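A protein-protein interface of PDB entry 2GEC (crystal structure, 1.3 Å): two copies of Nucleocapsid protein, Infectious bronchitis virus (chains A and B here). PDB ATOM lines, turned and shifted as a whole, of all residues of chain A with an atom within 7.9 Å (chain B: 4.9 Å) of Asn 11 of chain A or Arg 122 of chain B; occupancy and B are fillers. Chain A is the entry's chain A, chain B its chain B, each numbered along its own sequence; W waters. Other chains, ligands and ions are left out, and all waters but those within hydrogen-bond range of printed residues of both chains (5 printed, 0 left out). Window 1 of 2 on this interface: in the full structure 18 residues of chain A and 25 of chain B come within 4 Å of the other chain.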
ATOM      1  N   LYS A   5     -21.507  38.041 -28.521  1.00  0.00           N
ATOM      2  CA  LYS A   5     -22.128  37.650 -29.804  1.00  0.00           C
ATOM      3  C   LYS A   5     -22.535  36.180 -29.634  1.00  0.00           C
ATOM      4  O   LYS A   5     -21.702  35.274 -29.642  1.00  0.00           O
ATOM      5  CB  LYS A   5     -21.126  37.831 -30.998  1.00  0.00           C
ATOM      6  CG  LYS A   5     -20.822  39.281 -31.283  1.00  0.00           C
ATOM      7  CD  LYS A   5     -20.323  39.569 -32.688  1.00  0.00           C
ATOM      8  CE  LYS A   5     -19.174  38.750 -32.990  1.00  0.00           C
ATOM      9  NZ  LYS A   5     -18.553  39.208 -34.283  1.00  0.00           N
ATOM     10  N   VAL A   6     -23.833  35.991 -29.419  1.00  0.00           N
ATOM     11  CA  VAL A   6     -24.402  34.719 -29.186  1.00  0.00           C
ATOM     12  C   VAL A   6     -25.233  34.391 -30.469  1.00  0.00           C
ATOM     13  O   VAL A   6     -26.261  34.979 -30.690  1.00  0.00           O
ATOM     14  CB  VAL A   6     -25.278  34.705 -27.894  1.00  0.00           C
ATOM     15  CG1 VAL A   6     -25.808  33.264 -27.682  1.00  0.00           C
ATOM     16  CG2 VAL A   6     -24.432  35.185 -26.670  1.00  0.00           C
ATOM     17  N   GLY A   7     -24.694  33.523 -31.285  1.00  0.00           N
ATOM     18  CA  GLY A   7     -25.289  33.153 -32.564  1.00  0.00           C
ATOM     19  C   GLY A   7     -25.950  31.845 -32.692  1.00  0.00           C
ATOM     20  O   GLY A   7     -26.558  31.600 -33.736  1.00  0.00           O
ATOM     21  N   SER A   8     -25.861  30.997 -31.683  1.00  0.00           N
ATOM     22  CA  SER A   8     -26.468  29.680 -31.835  1.00  0.00           C
ATOM     23  C   SER A   8     -27.893  29.718 -31.366  1.00  0.00           C
ATOM     24  O   SER A   8     -28.187  30.326 -30.313  1.00  0.00           O
ATOM     25  CB  SER A   8     -25.649  28.693 -31.034  1.00  0.00           C
ATOM     26  OG  SER A   8     -26.294  27.443 -31.076  1.00  0.00           O
ATOM     27  N   SER A   9     -28.768  29.032 -32.097  1.00  0.00           N
ATOM     28  CA  SER A   9     -30.136  28.855 -31.685  1.00  0.00           C
ATOM     29  C   SER A   9     -30.216  27.758 -30.573  1.00  0.00           C
ATOM     30  O   SER A   9     -31.327  27.571 -30.007  1.00  0.00           O
ATOM     31  CB  SER A   9     -30.942  28.357 -32.914  1.00  0.00           C
ATOM     32  OG  SER A   9     -31.021  29.444 -33.857  1.00  0.00           O
ATOM     33  N   GLY A  10     -29.127  27.062 -30.272  1.00  0.00           N
ATOM     34  CA  GLY A  10     -29.162  26.097 -29.201  1.00  0.00           C
ATOM     35  C   GLY A  10     -28.061  25.091 -29.433  1.00  0.00           C
ATOM     36  O   GLY A  10     -27.817  24.670 -30.571  1.00  0.00           O
ATOM     37  N   ASN A  11     -27.358  24.706 -28.360  1.00  0.00           N
ATOM     38  CA  ASN A  11     -26.292  23.786 -28.502  1.00  0.00           C
ATOM     39  C   ASN A  11     -26.453  22.512 -27.736  1.00  0.00           C
ATOM     40  O   ASN A  11     -25.499  21.772 -27.641  1.00  0.00           O
ATOM     41  CB  ASN A  11     -24.960  24.459 -28.093  1.00  0.00           C
ATOM     42  CG  ASN A  11     -24.533  25.560 -29.010  1.00  0.00           C
ATOM     43  OD1 ASN A  11     -23.829  26.491 -28.591  1.00  0.00           O
ATOM     44  ND2 ASN A  11     -24.780  25.388 -30.267  1.00  0.00           N
ATOM     45  N   ALA A  12     -27.634  22.237 -27.198  1.00  0.00           N
ATOM     46  CA  ALA A  12     -27.826  20.981 -26.474  1.00  0.00           C
ATOM     47  C   ALA A  12     -28.297  19.958 -27.460  1.00  0.00           C
ATOM     48  O   ALA A  12     -29.341  20.131 -28.090  1.00  0.00           O
ATOM     49  CB  ALA A  12     -28.795  21.120 -25.325  1.00  0.00           C
ATOM     50  N   SER A  13     -27.549  18.929 -27.653  1.00  0.00           N
ATOM     51  CA  SER A  13     -27.991  17.860 -28.524  1.00  0.00           C
ATOM     52  C   SER A  13     -29.289  17.249 -28.068  1.00  0.00           C
ATOM     53  O   SER A  13     -29.530  17.114 -26.869  1.00  0.00           O
ATOM     54  CB  SER A  13     -26.891  16.777 -28.494  1.00  0.00           C
ATOM     55  OG  SER A  13     -27.262  15.652 -29.331  1.00  0.00           O
ATOM     56  N   TRP A  14     -30.123  16.773 -29.014  1.00  0.00           N
ATOM     57  CA  TRP A  14     -31.286  16.027 -28.579  1.00  0.00           C
ATOM     58  C   TRP A  14     -30.966  14.722 -27.903  1.00  0.00           C
ATOM     59  O   TRP A  14     -31.762  14.234 -27.123  1.00  0.00           O
ATOM     60  CB  TRP A  14     -32.120  15.666 -29.823  1.00  0.00           C
ATOM     61  CG  TRP A  14     -33.001  16.797 -30.242  1.00  0.00           C
ATOM     62  CD1 TRP A  14     -32.864  17.581 -31.352  1.00  0.00           C
ATOM     63  CD2 TRP A  14     -34.207  17.282 -29.563  1.00  0.00           C
ATOM     64  NE1 TRP A  14     -33.907  18.491 -31.431  1.00  0.00           N
ATOM     65  CE2 TRP A  14     -34.711  18.359 -30.312  1.00  0.00           C
ATOM     66  CE3 TRP A  14     -34.843  16.902 -28.393  1.00  0.00           C
ATOM     67  CZ2 TRP A  14     -35.909  19.005 -30.002  1.00  0.00           C
ATOM     68  CZ3 TRP A  14     -36.043  17.562 -28.024  1.00  0.00           C
ATOM     69  CH2 TRP A  14     -36.551  18.594 -28.813  1.00  0.00           C
ATOM     70  N   TYR A  49     -23.965  15.722 -37.962  1.00  0.00           N
ATOM     71  CA  TYR A  49     -22.552  15.570 -37.560  1.00  0.00           C
ATOM     72  C   TYR A  49     -22.425  15.245 -36.118  1.00  0.00           C
ATOM     73  O   TYR A  49     -23.296  15.549 -35.337  1.00  0.00           O
ATOM     74  CB  TYR A  49     -21.723  16.831 -37.884  1.00  0.00           C
ATOM     75  CG  TYR A  49     -22.200  18.065 -37.098  1.00  0.00           C
ATOM     76  CD1 TYR A  49     -23.201  18.896 -37.609  1.00  0.00           C
ATOM     77  CD2 TYR A  49     -21.628  18.399 -35.870  1.00  0.00           C
ATOM     78  CE1 TYR A  49     -23.604  20.028 -36.903  1.00  0.00           C
ATOM     79  CE2 TYR A  49     -22.049  19.502 -35.171  1.00  0.00           C
ATOM     80  CZ  TYR A  49     -23.025  20.292 -35.673  1.00  0.00           C
ATOM     81  OH  TYR A  49     -23.419  21.414 -34.944  1.00  0.00           O
ATOM     82  N   ARG A  51     -19.878  15.877 -32.956  1.00  0.00           N
ATOM     83  CA  ARG A  51     -18.884  16.919 -32.586  1.00  0.00           C
ATOM     84  C   ARG A  51     -18.234  16.606 -31.248  1.00  0.00           C
ATOM     85  O   ARG A  51     -18.908  16.352 -30.266  1.00  0.00           O
ATOM     86  CB  ARG A  51     -19.575  18.281 -32.483  1.00  0.00           C
ATOM     87  CG  ARG A  51     -18.542  19.462 -32.174  1.00  0.00           C
ATOM     88  CD  ARG A  51     -19.310  20.740 -32.139  1.00  0.00           C
ATOM     89  NE  ARG A  51     -18.449  21.877 -31.697  1.00  0.00           N
ATOM     90  CZ  ARG A  51     -18.217  22.236 -30.441  1.00  0.00           C
ATOM     91  NH1 ARG A  51     -18.624  21.484 -29.418  1.00  0.00           N
ATOM     92  NH2 ARG A  51     -17.574  23.401 -30.173  1.00  0.00           N
ATOM     93  N   GLN A  53     -16.257  16.943 -27.742  1.00  0.00           N
ATOM     94  CA  GLN A  53     -16.150  17.831 -26.580  1.00  0.00           C
ATOM     95  C   GLN A  53     -15.135  17.250 -25.636  1.00  0.00           C
ATOM     96  O   GLN A  53     -15.258  16.115 -25.198  1.00  0.00           O
ATOM     97  CB  GLN A  53     -17.544  17.916 -25.859  1.00  0.00           C
ATOM     98  CG  GLN A  53     -17.535  18.967 -24.780  1.00  0.00           C
ATOM     99  CD  GLN A  53     -18.506  18.710 -23.804  1.00  0.00           C
ATOM    100  OE1 GLN A  53     -19.661  18.932 -24.071  1.00  0.00           O
ATOM    101  NE2 GLN A  53     -18.040  18.327 -22.534  1.00  0.00           N
ATOM    102  N   TYR A  71     -21.223  14.495 -29.465  1.00  0.00           N
ATOM    103  CA  TYR A  71     -22.678  14.740 -29.502  1.00  0.00           C
ATOM    104  C   TYR A  71     -23.138  14.922 -30.936  1.00  0.00           C
ATOM    105  O   TYR A  71     -22.463  15.516 -31.751  1.00  0.00           O
ATOM    106  CB  TYR A  71     -22.935  16.059 -28.770  1.00  0.00           C
ATOM    107  CG  TYR A  71     -22.753  15.956 -27.265  1.00  0.00           C
ATOM    108  CD1 TYR A  71     -23.800  15.561 -26.438  1.00  0.00           C
ATOM    109  CD2 TYR A  71     -21.520  16.223 -26.690  1.00  0.00           C
ATOM    110  CE1 TYR A  71     -23.679  15.545 -25.043  1.00  0.00           C
ATOM    111  CE2 TYR A  71     -21.362  16.087 -25.310  1.00  0.00           C
ATOM    112  CZ  TYR A  71     -22.444  15.857 -24.509  1.00  0.00           C
ATOM    113  OH  TYR A  71     -22.328  15.802 -23.133  1.00  0.00           O
ATOM    114  N   PHE A  72     -24.331  14.424 -31.234  1.00  0.00           N
ATOM    115  CA  PHE A  72     -24.897  14.528 -32.557  1.00  0.00           C
ATOM    116  C   PHE A  72     -25.819  15.772 -32.726  1.00  0.00           C
ATOM    117  O   PHE A  72     -26.664  16.060 -31.882  1.00  0.00           O
ATOM    118  CB  PHE A  72     -25.738  13.281 -32.831  1.00  0.00           C
ATOM    119  CG  PHE A  72     -26.421  13.354 -34.168  1.00  0.00           C
ATOM    120  CD1 PHE A  72     -25.752  13.037 -35.284  1.00  0.00           C
ATOM    121  CD2 PHE A  72     -27.752  13.789 -34.277  1.00  0.00           C
ATOM    122  CE1 PHE A  72     -26.354  13.149 -36.525  1.00  0.00           C
ATOM    123  CE2 PHE A  72     -28.351  13.955 -35.476  1.00  0.00           C
ATOM    124  CZ  PHE A  72     -27.681  13.593 -36.641  1.00  0.00           C
ATOM    125  N   TYR A  73     -25.673  16.415 -33.883  1.00  0.00           N
ATOM    126  CA  TYR A  73     -26.519  17.506 -34.266  1.00  0.00           C
ATOM    127  C   TYR A  73     -26.954  17.353 -35.723  1.00  0.00           C
ATOM    128  O   TYR A  73     -26.157  16.939 -36.549  1.00  0.00           O
ATOM    129  CB  TYR A  73     -25.722  18.830 -34.148  1.00  0.00           C
ATOM    130  CG  TYR A  73     -25.322  19.122 -32.725  1.00  0.00           C
ATOM    131  CD1 TYR A  73     -26.202  19.798 -31.886  1.00  0.00           C
ATOM    132  CD2 TYR A  73     -24.103  18.750 -32.248  1.00  0.00           C
ATOM    133  CE1 TYR A  73     -25.824  20.042 -30.578  1.00  0.00           C
ATOM    134  CE2 TYR A  73     -23.703  19.009 -30.953  1.00  0.00           C
ATOM    135  CZ  TYR A  73     -24.590  19.593 -30.137  1.00  0.00           C
ATOM    136  OH  TYR A  73     -24.199  19.863 -28.803  1.00  0.00           O
ATOM    137  N   THR A  77     -27.686  22.909 -37.433  1.00  0.00           N
ATOM    138  CA  THR A  77     -27.999  23.164 -36.019  1.00  0.00           C
ATOM    139  C   THR A  77     -26.742  22.994 -35.235  1.00  0.00           C
ATOM    140  O   THR A  77     -25.786  22.363 -35.712  1.00  0.00           O
ATOM    141  CB  THR A  77     -29.085  22.196 -35.473  1.00  0.00           C
ATOM    142  OG1 THR A  77     -28.511  20.880 -35.233  1.00  0.00           O
ATOM    143  CG2 THR A  77     -30.281  22.058 -36.465  1.00  0.00           C
ATOM    144  N   GLY A  78     -26.758  23.449 -33.985  1.00  0.00           N
ATOM    145  CA  GLY A  78     -25.671  23.195 -33.031  1.00  0.00           C
ATOM    146  C   GLY A  78     -24.482  24.091 -33.279  1.00  0.00           C
ATOM    147  O   GLY A  78     -24.555  25.039 -34.011  1.00  0.00           O
ATOM    148  N   PRO A  79     -23.371  23.777 -32.637  1.00  0.00           N
ATOM    149  CA  PRO A  79     -22.199  24.687 -32.663  1.00  0.00           C
ATOM    150  C   PRO A  79     -21.666  24.866 -34.081  1.00  0.00           C
ATOM    151  O   PRO A  79     -21.184  25.966 -34.449  1.00  0.00           O
ATOM    152  CB  PRO A  79     -21.155  23.944 -31.798  1.00  0.00           C
ATOM    153  CG  PRO A  79     -22.000  23.219 -30.771  1.00  0.00           C
ATOM    154  CD  PRO A  79     -23.233  22.704 -31.629  1.00  0.00           C
ATOM    155  N   ALA A  80     -21.754  23.838 -34.905  1.00  0.00           N
ATOM    156  CA  ALA A  80     -21.281  23.924 -36.283  1.00  0.00           C
ATOM    157  C   ALA A  80     -22.407  24.073 -37.282  1.00  0.00           C
ATOM    158  O   ALA A  80     -22.308  23.618 -38.417  1.00  0.00           O
ATOM    159  CB  ALA A  80     -20.473  22.659 -36.623  1.00  0.00           C
ATOM    160  N   ALA A  81     -23.450  24.760 -36.884  1.00  0.00           N
ATOM    161  CA  ALA A  81     -24.602  25.033 -37.729  1.00  0.00           C
ATOM    162  C   ALA A  81     -24.258  25.699 -39.043  1.00  0.00           C
ATOM    163  O   ALA A  81     -24.939  25.419 -40.031  1.00  0.00           O
ATOM    164  CB  ALA A  81     -25.631  25.882 -36.980  1.00  0.00           C
ATOM    165  N   THR A 110     -32.630  21.916 -31.962  1.00  0.00           N
ATOM    166  CA  THR A 110     -31.892  21.322 -30.866  1.00  0.00           C
ATOM    167  C   THR A 110     -32.810  21.254 -29.639  1.00  0.00           C
ATOM    168  O   THR A 110     -33.947  21.677 -29.656  1.00  0.00           O
ATOM    169  CB  THR A 110     -30.598  22.094 -30.490  1.00  0.00           C
ATOM    170  OG1 THR A 110     -30.950  23.429 -30.129  1.00  0.00           O
ATOM    171  CG2 THR A 110     -29.657  22.125 -31.647  1.00  0.00           C
ATOM    172  N   ARG A 111     -32.302  20.711 -28.573  1.00  0.00           N
ATOM    173  CA  ARG A 111     -33.117  20.397 -27.377  1.00  0.00           C
ATOM    174  C   ARG A 111     -33.055  21.510 -26.345  1.00  0.00           C
ATOM    175  O   ARG A 111     -31.973  21.982 -26.001  1.00  0.00           O
ATOM    176  CB  ARG A 111     -32.562  19.156 -26.712  1.00  0.00           C
ATOM    177  CG  ARG A 111     -33.330  18.699 -25.467  1.00  0.00           C
ATOM    178  CD  ARG A 111     -32.860  17.310 -25.014  1.00  0.00           C
ATOM    179  NE  ARG A 111     -31.411  17.204 -24.857  1.00  0.00           N
ATOM    180  CZ  ARG A 111     -30.766  17.538 -23.742  1.00  0.00           C
ATOM    181  NH1 ARG A 111     -31.426  17.947 -22.607  1.00  0.00           N
ATOM    182  NH2 ARG A 111     -29.453  17.555 -23.714  1.00  0.00           N
ATOM    183  N   ASP A 112     -34.197  21.918 -25.819  1.00  0.00           N
ATOM    184  CA  ASP A 112     -34.221  22.780 -24.604  1.00  0.00           C
ATOM    185  C   ASP A 112     -34.054  21.918 -23.361  1.00  0.00           C
ATOM    186  O   ASP A 112     -34.985  21.173 -23.023  1.00  0.00           O
ATOM    187  CB  ASP A 112     -35.540  23.555 -24.572  1.00  0.00           C
ATOM    188  CG  ASP A 112     -35.679  24.448 -23.305  1.00  0.00           C
ATOM    189  OD1 ASP A 112     -34.745  24.425 -22.472  1.00  0.00           O
ATOM    190  OD2 ASP A 112     -36.684  25.130 -23.256  1.00  0.00           O
ATOM    191  N   PRO A 113     -32.897  21.953 -22.691  1.00  0.00           N
ATOM    192  CA  PRO A 113     -32.714  21.059 -21.599  1.00  0.00           C
ATOM    193  C   PRO A 113     -33.625  21.311 -20.415  1.00  0.00           C
ATOM    194  O   PRO A 113     -33.818  20.398 -19.580  1.00  0.00           O
ATOM    195  CB  PRO A 113     -31.204  21.247 -21.174  1.00  0.00           C
ATOM    196  CG  PRO A 113     -30.854  22.680 -21.729  1.00  0.00           C
ATOM    197  CD  PRO A 113     -31.751  22.895 -22.872  1.00  0.00           C
ATOM    198  N   VAL B  35     -18.014  27.583 -20.061  1.00  0.00           N
ATOM    199  CA  VAL B  35     -17.903  28.961 -20.478  1.00  0.00           C
ATOM    200  C   VAL B  35     -19.007  29.189 -21.523  1.00  0.00           C
ATOM    201  O   VAL B  35     -19.108  28.420 -22.533  1.00  0.00           O
ATOM    202  CB  VAL B  35     -16.495  29.232 -21.109  1.00  0.00           C
ATOM    203  CG1 VAL B  35     -16.460  30.672 -21.657  1.00  0.00           C
ATOM    204  CG2 VAL B  35     -15.405  28.977 -20.085  1.00  0.00           C
ATOM    205  N   PRO B  36     -19.824  30.233 -21.354  1.00  0.00           N
ATOM    206  CA  PRO B  36     -20.873  30.499 -22.376  1.00  0.00           C
ATOM    207  C   PRO B  36     -20.282  30.808 -23.756  1.00  0.00           C
ATOM    208  O   PRO B  36     -19.204  31.405 -23.840  1.00  0.00           O
ATOM    209  CB  PRO B  36     -21.597  31.675 -21.774  1.00  0.00           C
ATOM    210  CG  PRO B  36     -21.292  31.662 -20.259  1.00  0.00           C
ATOM    211  CD  PRO B  36     -19.894  31.194 -20.237  1.00  0.00           C
ATOM    212  N   ASP B  37     -21.026  30.566 -24.842  1.00  0.00           N
ATOM    213  CA  ASP B  37     -20.595  31.033 -26.150  1.00  0.00           C
ATOM    214  C   ASP B  37     -20.568  32.554 -26.217  1.00  0.00           C
ATOM    215  O   ASP B  37     -21.444  33.274 -25.678  1.00  0.00           O
ATOM    216  CB  ASP B  37     -21.641  30.638 -27.213  1.00  0.00           C
ATOM    217  CG  ASP B  37     -21.628  29.202 -27.577  1.00  0.00           C
ATOM    218  OD1 ASP B  37     -22.472  28.939 -28.538  1.00  0.00           O
ATOM    219  OD2 ASP B  37     -20.820  28.364 -27.066  1.00  0.00           O
ATOM    220  N   PRO B 120     -28.621  35.216 -23.717  1.00  0.00           N
ATOM    221  CA  PRO B 120     -28.810  33.777 -23.545  1.00  0.00           C
ATOM    222  C   PRO B 120     -27.528  32.980 -23.314  1.00  0.00           C
ATOM    223  O   PRO B 120     -26.529  33.288 -23.913  1.00  0.00           O
ATOM    224  CB  PRO B 120     -29.523  33.345 -24.862  1.00  0.00           C
ATOM    225  CG  PRO B 120     -29.897  34.494 -25.581  1.00  0.00           C
ATOM    226  CD  PRO B 120     -28.967  35.641 -25.083  1.00  0.00           C
ATOM    227  N   LEU B 121     -27.635  31.910 -22.513  1.00  0.00           N
ATOM    228  CA  LEU B 121     -26.528  31.006 -22.355  1.00  0.00           C
ATOM    229  C   LEU B 121     -26.584  29.954 -23.473  1.00  0.00           C
ATOM    230  O   LEU B 121     -27.682  29.354 -23.765  1.00  0.00           O
ATOM    231  CB  LEU B 121     -26.712  30.235 -21.050  1.00  0.00           C
ATOM    232  CG  LEU B 121     -26.350  31.100 -19.835  1.00  0.00           C
ATOM    233  CD1 LEU B 121     -26.734  30.377 -18.534  1.00  0.00           C
ATOM    234  CD2 LEU B 121     -24.780  31.398 -19.807  1.00  0.00           C
ATOM    235  N   ARG B 122     -25.472  29.727 -24.128  1.00  0.00           N
ATOM    236  CA  ARG B 122     -25.357  28.662 -25.058  1.00  0.00           C
ATOM    237  C   ARG B 122     -24.071  28.013 -24.680  1.00  0.00           C
ATOM    238  O   ARG B 122     -23.078  28.718 -24.518  1.00  0.00           O
ATOM    239  CB  ARG B 122     -25.315  29.237 -26.515  1.00  0.00           C
ATOM    240  CG  ARG B 122     -26.645  29.909 -26.960  1.00  0.00           C
ATOM    241  CD  ARG B 122     -27.680  28.845 -27.193  1.00  0.00           C
ATOM    242  NE  ARG B 122     -28.911  29.572 -27.725  1.00  0.00           N
ATOM    243  CZ  ARG B 122     -29.915  30.107 -27.020  1.00  0.00           C
ATOM    244  NH1 ARG B 122     -29.852  30.044 -25.695  1.00  0.00           N
ATOM    245  NH2 ARG B 122     -30.937  30.746 -27.621  1.00  0.00           N
ATOM    246  N   PHE B 123     -24.080  26.682 -24.584  1.00  0.00           N
ATOM    247  CA  PHE B 123     -22.862  25.968 -24.112  1.00  0.00           C
ATOM    248  C   PHE B 123     -22.322  25.002 -25.168  1.00  0.00           C
ATOM    249  O   PHE B 123     -22.731  23.905 -25.222  1.00  0.00           O
ATOM    250  CB  PHE B 123     -23.174  25.177 -22.824  1.00  0.00           C
ATOM    251  CG  PHE B 123     -23.369  26.043 -21.613  1.00  0.00           C
ATOM    252  CD1 PHE B 123     -24.636  26.170 -21.074  1.00  0.00           C
ATOM    253  CD2 PHE B 123     -22.281  26.752 -21.049  1.00  0.00           C
ATOM    254  CE1 PHE B 123     -24.808  26.961 -19.933  1.00  0.00           C
ATOM    255  CE2 PHE B 123     -22.469  27.499 -19.908  1.00  0.00           C
ATOM    256  CZ  PHE B 123     -23.738  27.612 -19.360  1.00  0.00           C
ATOM    257  N   SER B 124     -21.479  25.469 -26.083  1.00  0.00           N
ATOM    258  CA  SER B 124     -20.967  24.556 -27.146  1.00  0.00           C
ATOM    259  C   SER B 124     -20.186  23.372 -26.531  1.00  0.00           C
ATOM    260  O   SER B 124     -20.215  22.210 -26.988  1.00  0.00           O
ATOM    261  CB  SER B 124     -20.061  25.305 -28.130  1.00  0.00           C
ATOM    262  OG  SER B 124     -20.817  26.255 -28.907  1.00  0.00           O
ATOM    263  N   PHE B 136     -35.074  28.786 -21.246  1.00  0.00           N
ATOM    264  CA  PHE B 136     -34.571  29.094 -22.626  1.00  0.00           C
ATOM    265  C   PHE B 136     -34.962  30.470 -23.048  1.00  0.00           C
ATOM    266  O   PHE B 136     -36.140  30.845 -22.981  1.00  0.00           O
ATOM    267  CB  PHE B 136     -35.136  28.045 -23.615  1.00  0.00           C
ATOM    268  CG  PHE B 136     -34.634  28.204 -25.049  1.00  0.00           C
ATOM    269  CD1 PHE B 136     -33.335  27.840 -25.394  1.00  0.00           C
ATOM    270  CD2 PHE B 136     -35.427  28.802 -26.005  1.00  0.00           C
ATOM    271  CE1 PHE B 136     -32.853  28.017 -26.730  1.00  0.00           C
ATOM    272  CE2 PHE B 136     -34.971  28.921 -27.338  1.00  0.00           C
ATOM    273  CZ  PHE B 136     -33.663  28.537 -27.652  1.00  0.00           C
ATOM    274  N   ILE B 137     -33.984  31.171 -23.592  1.00  0.00           N
ATOM    275  CA  ILE B 137     -34.209  32.515 -24.128  1.00  0.00           C
ATOM    276  C   ILE B 137     -33.863  32.433 -25.592  1.00  0.00           C
ATOM    277  O   ILE B 137     -32.705  32.209 -25.916  1.00  0.00           O
ATOM    278  CB  ILE B 137     -33.249  33.562 -23.479  1.00  0.00           C
ATOM    279  CG1 ILE B 137     -33.407  33.655 -21.950  1.00  0.00           C
ATOM    280  CG2 ILE B 137     -33.440  34.981 -24.160  1.00  0.00           C
ATOM    281  CD1 ILE B 137     -32.366  34.642 -21.335  1.00  0.00           C
ATOM    282  N   PRO B 138     -34.856  32.549 -26.477  1.00  0.00           N
ATOM    283  CA  PRO B 138     -34.536  32.492 -27.897  1.00  0.00           C
ATOM    284  C   PRO B 138     -33.739  33.720 -28.367  1.00  0.00           C
ATOM    285  O   PRO B 138     -33.759  34.782 -27.719  1.00  0.00           O
ATOM    286  CB  PRO B 138     -35.905  32.574 -28.575  1.00  0.00           C
ATOM    287  CG  PRO B 138     -36.914  32.271 -27.557  1.00  0.00           C
ATOM    288  CD  PRO B 138     -36.298  32.678 -26.225  1.00  0.00           C
ATOM    289  N   LEU B 139     -32.950  33.498 -29.406  1.00  0.00           N
ATOM    290  CA  LEU B 139     -32.227  34.540 -30.159  1.00  0.00           C
ATOM    291  C   LEU B 139     -30.869  34.580 -29.474  1.00  0.00           C
ATOM    292  O   LEU B 139     -29.918  33.727 -29.762  1.00  0.00           O
ATOM    293  CB  LEU B 139     -33.066  35.867 -30.429  1.00  0.00           C
ATOM    294  CG  LEU B 139     -33.366  37.119 -29.562  1.00  0.00           C
ATOM    295  CD1 LEU B 139     -32.239  38.071 -29.565  1.00  0.00           C
ATOM    296  CD2 LEU B 139     -34.690  37.891 -29.878  1.00  0.00           C
ATOM    297  OXT LEU B 139     -30.742  35.334 -28.524  1.00  0.00           O
HETATM  298  O   HOH W   1     -27.791  37.008 -28.920  1.00  0.00           O
HETATM  299  O   HOH W   2     -20.369  19.543 -26.545  1.00  0.00           O
HETATM  300  O   HOH W   3     -32.872  30.673 -30.469  1.00  0.00           O
HETATM  301  O   HOH W   4     -37.138  26.728 -21.110  1.00  0.00           O
HETATM  302  O   HOH W   5     -26.893  25.370 -25.241  1.00  0.00           O
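The side-chain carboxylate of Asp 37 of chain B lies close to the side-chain amide oxygen of Asn 11 of chain A (2.8 Å).
The side-chain amide oxygen of Asn 11 of chain A is in hydrogen-bond range of the side-chain hydroxyl of Ser 124 of chain B (3.0 Å).
The guanidinium group (NE) of Arg 122 of chain B is in hydrogen-bond range of the backbone carbonyl oxygen (O) of Ser 8 of chain A, at 2.8 Å.
The backbone carbonyl oxygen of Ser 124 of chain B lies within hydrogen-bond range of the guanidinium group of Arg 51 of chain A, 3.0 Å away.
The guanidinium group (NH2) of Arg 122 of chain B lies within salt-bridge range of the chain-end carboxylate (O) of Leu 139 of chain B, at 3.8 Å.
The side-chain hydroxyl (OG) of Ser 8 of chain A sits at hydrogen-bond distance from the side-chain amide nitrogen (ND2) of Asn 11 of chain A, at 2.7 Å.
The backbone carbonyl oxygen (O) of Tyr 71 of chain A is in hydrogen-bond range of the backbone NH (N) of Arg 51 of chain A, at 2.9 Å.
Among the printed residues, pairs that only touch across the chains: Val 6 of chain A with Asp 37 of chain B (3.7 Å), Val 6 of chain A with Pro 120 of chain B (3.8 Å), Val 6 of chain A with Arg 122 of chain B (3.5 Å), Val 6 of chain A with Leu 139 of chain B (3.98 Å), Ser 8 of chain A with Leu 139 of chain B (3.9 Å), Ser 9 of chain A with Arg 122 of chain B (3.6 Å), Ser 9 of chain A with Phe 136 of chain B (3.5 Å), Gly 10 of chain A with Arg 122 of chain B (3.6 Å), Asn 11 of chain A with Arg 122 of chain B (3.7 Å), Asn 11 of chain A with Phe 123 of chain B (3.7 Å), Pro 79 of chain A with Ser 124 of chain B (3.7 Å) and Asp 112 of chain A with Phe 136 of chain B (3.3 Å).
Of the printed residues of chain B, Gly 10 of chain A touches Arg 122 (3.6 Å).
Of the printed residues of chain B, Asn 11 of chain A touches Asp 37, Arg 122, Phe 123 and Ser 124.
Trp 14 of chain A touches none of the printed residues of chain B.
Pro 113 of chain A touches none of the printed residues of chain B.
Printed residues of chain A within 4 Å of Asp 37 of chain B: Val 6 (3.7 Å) and Asn 11 (2.8 Å).
Printed residues of chain A within 4 Å of Pro 120 of chain B: Val 6.
Printed residues of chain A within 4 Å of Leu 139 of chain B: Val 6 and Ser 8.
Of the 25 printed residues of chain A, 8 touch a printed residue of chain B.
Hydrophobic or aromatic side chains of chain A that line the printed part of chain B: Val 6 and Pro 79.
Of the 12 printed residues of chain B, 7 touch a printed residue of chain A.
Printed residues of chain B that touch a printed residue of chain A: Asp 37, Pro 120, Arg 122, Phe 123, Ser 124, Phe 136 and Leu 139.
Hydrophobic or aromatic side chains of chain B within 4 Å of the printed part of chain A: Phe 136.
Among the printed residues, 16 pairs touch across the chains.
Among the printed residues, no Asp or Glu carboxylate lies within 4 Å of a Lys or Arg side-chain nitrogen of the other chain.
No position is printed for both chains.
Water W2 lies within hydrogen-bond range of OE1 of Gln 53 of chain A (2.6 Å) and O of Ser 124 of chain B (2.7 Å).
Water W4 bridges the side-chain carboxylate (OD2) of Asp 112 of chain A and the backbone NH (N) of Phe 136 of chain B.
Water W3 lies within hydrogen-bond range of N of Leu 139 of chain B, NH2 of Arg 122 of chain B and O of Ser 9 of chain A.
Water W1 lies within hydrogen-bond range of O of Val 6 of chain A (3.1 Å) and OXT of Leu 139 of chain B (3.4 Å).
Water W5 lies within hydrogen-bond range of N of Phe 123 of chain B and N of Asn 11 of chain A.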
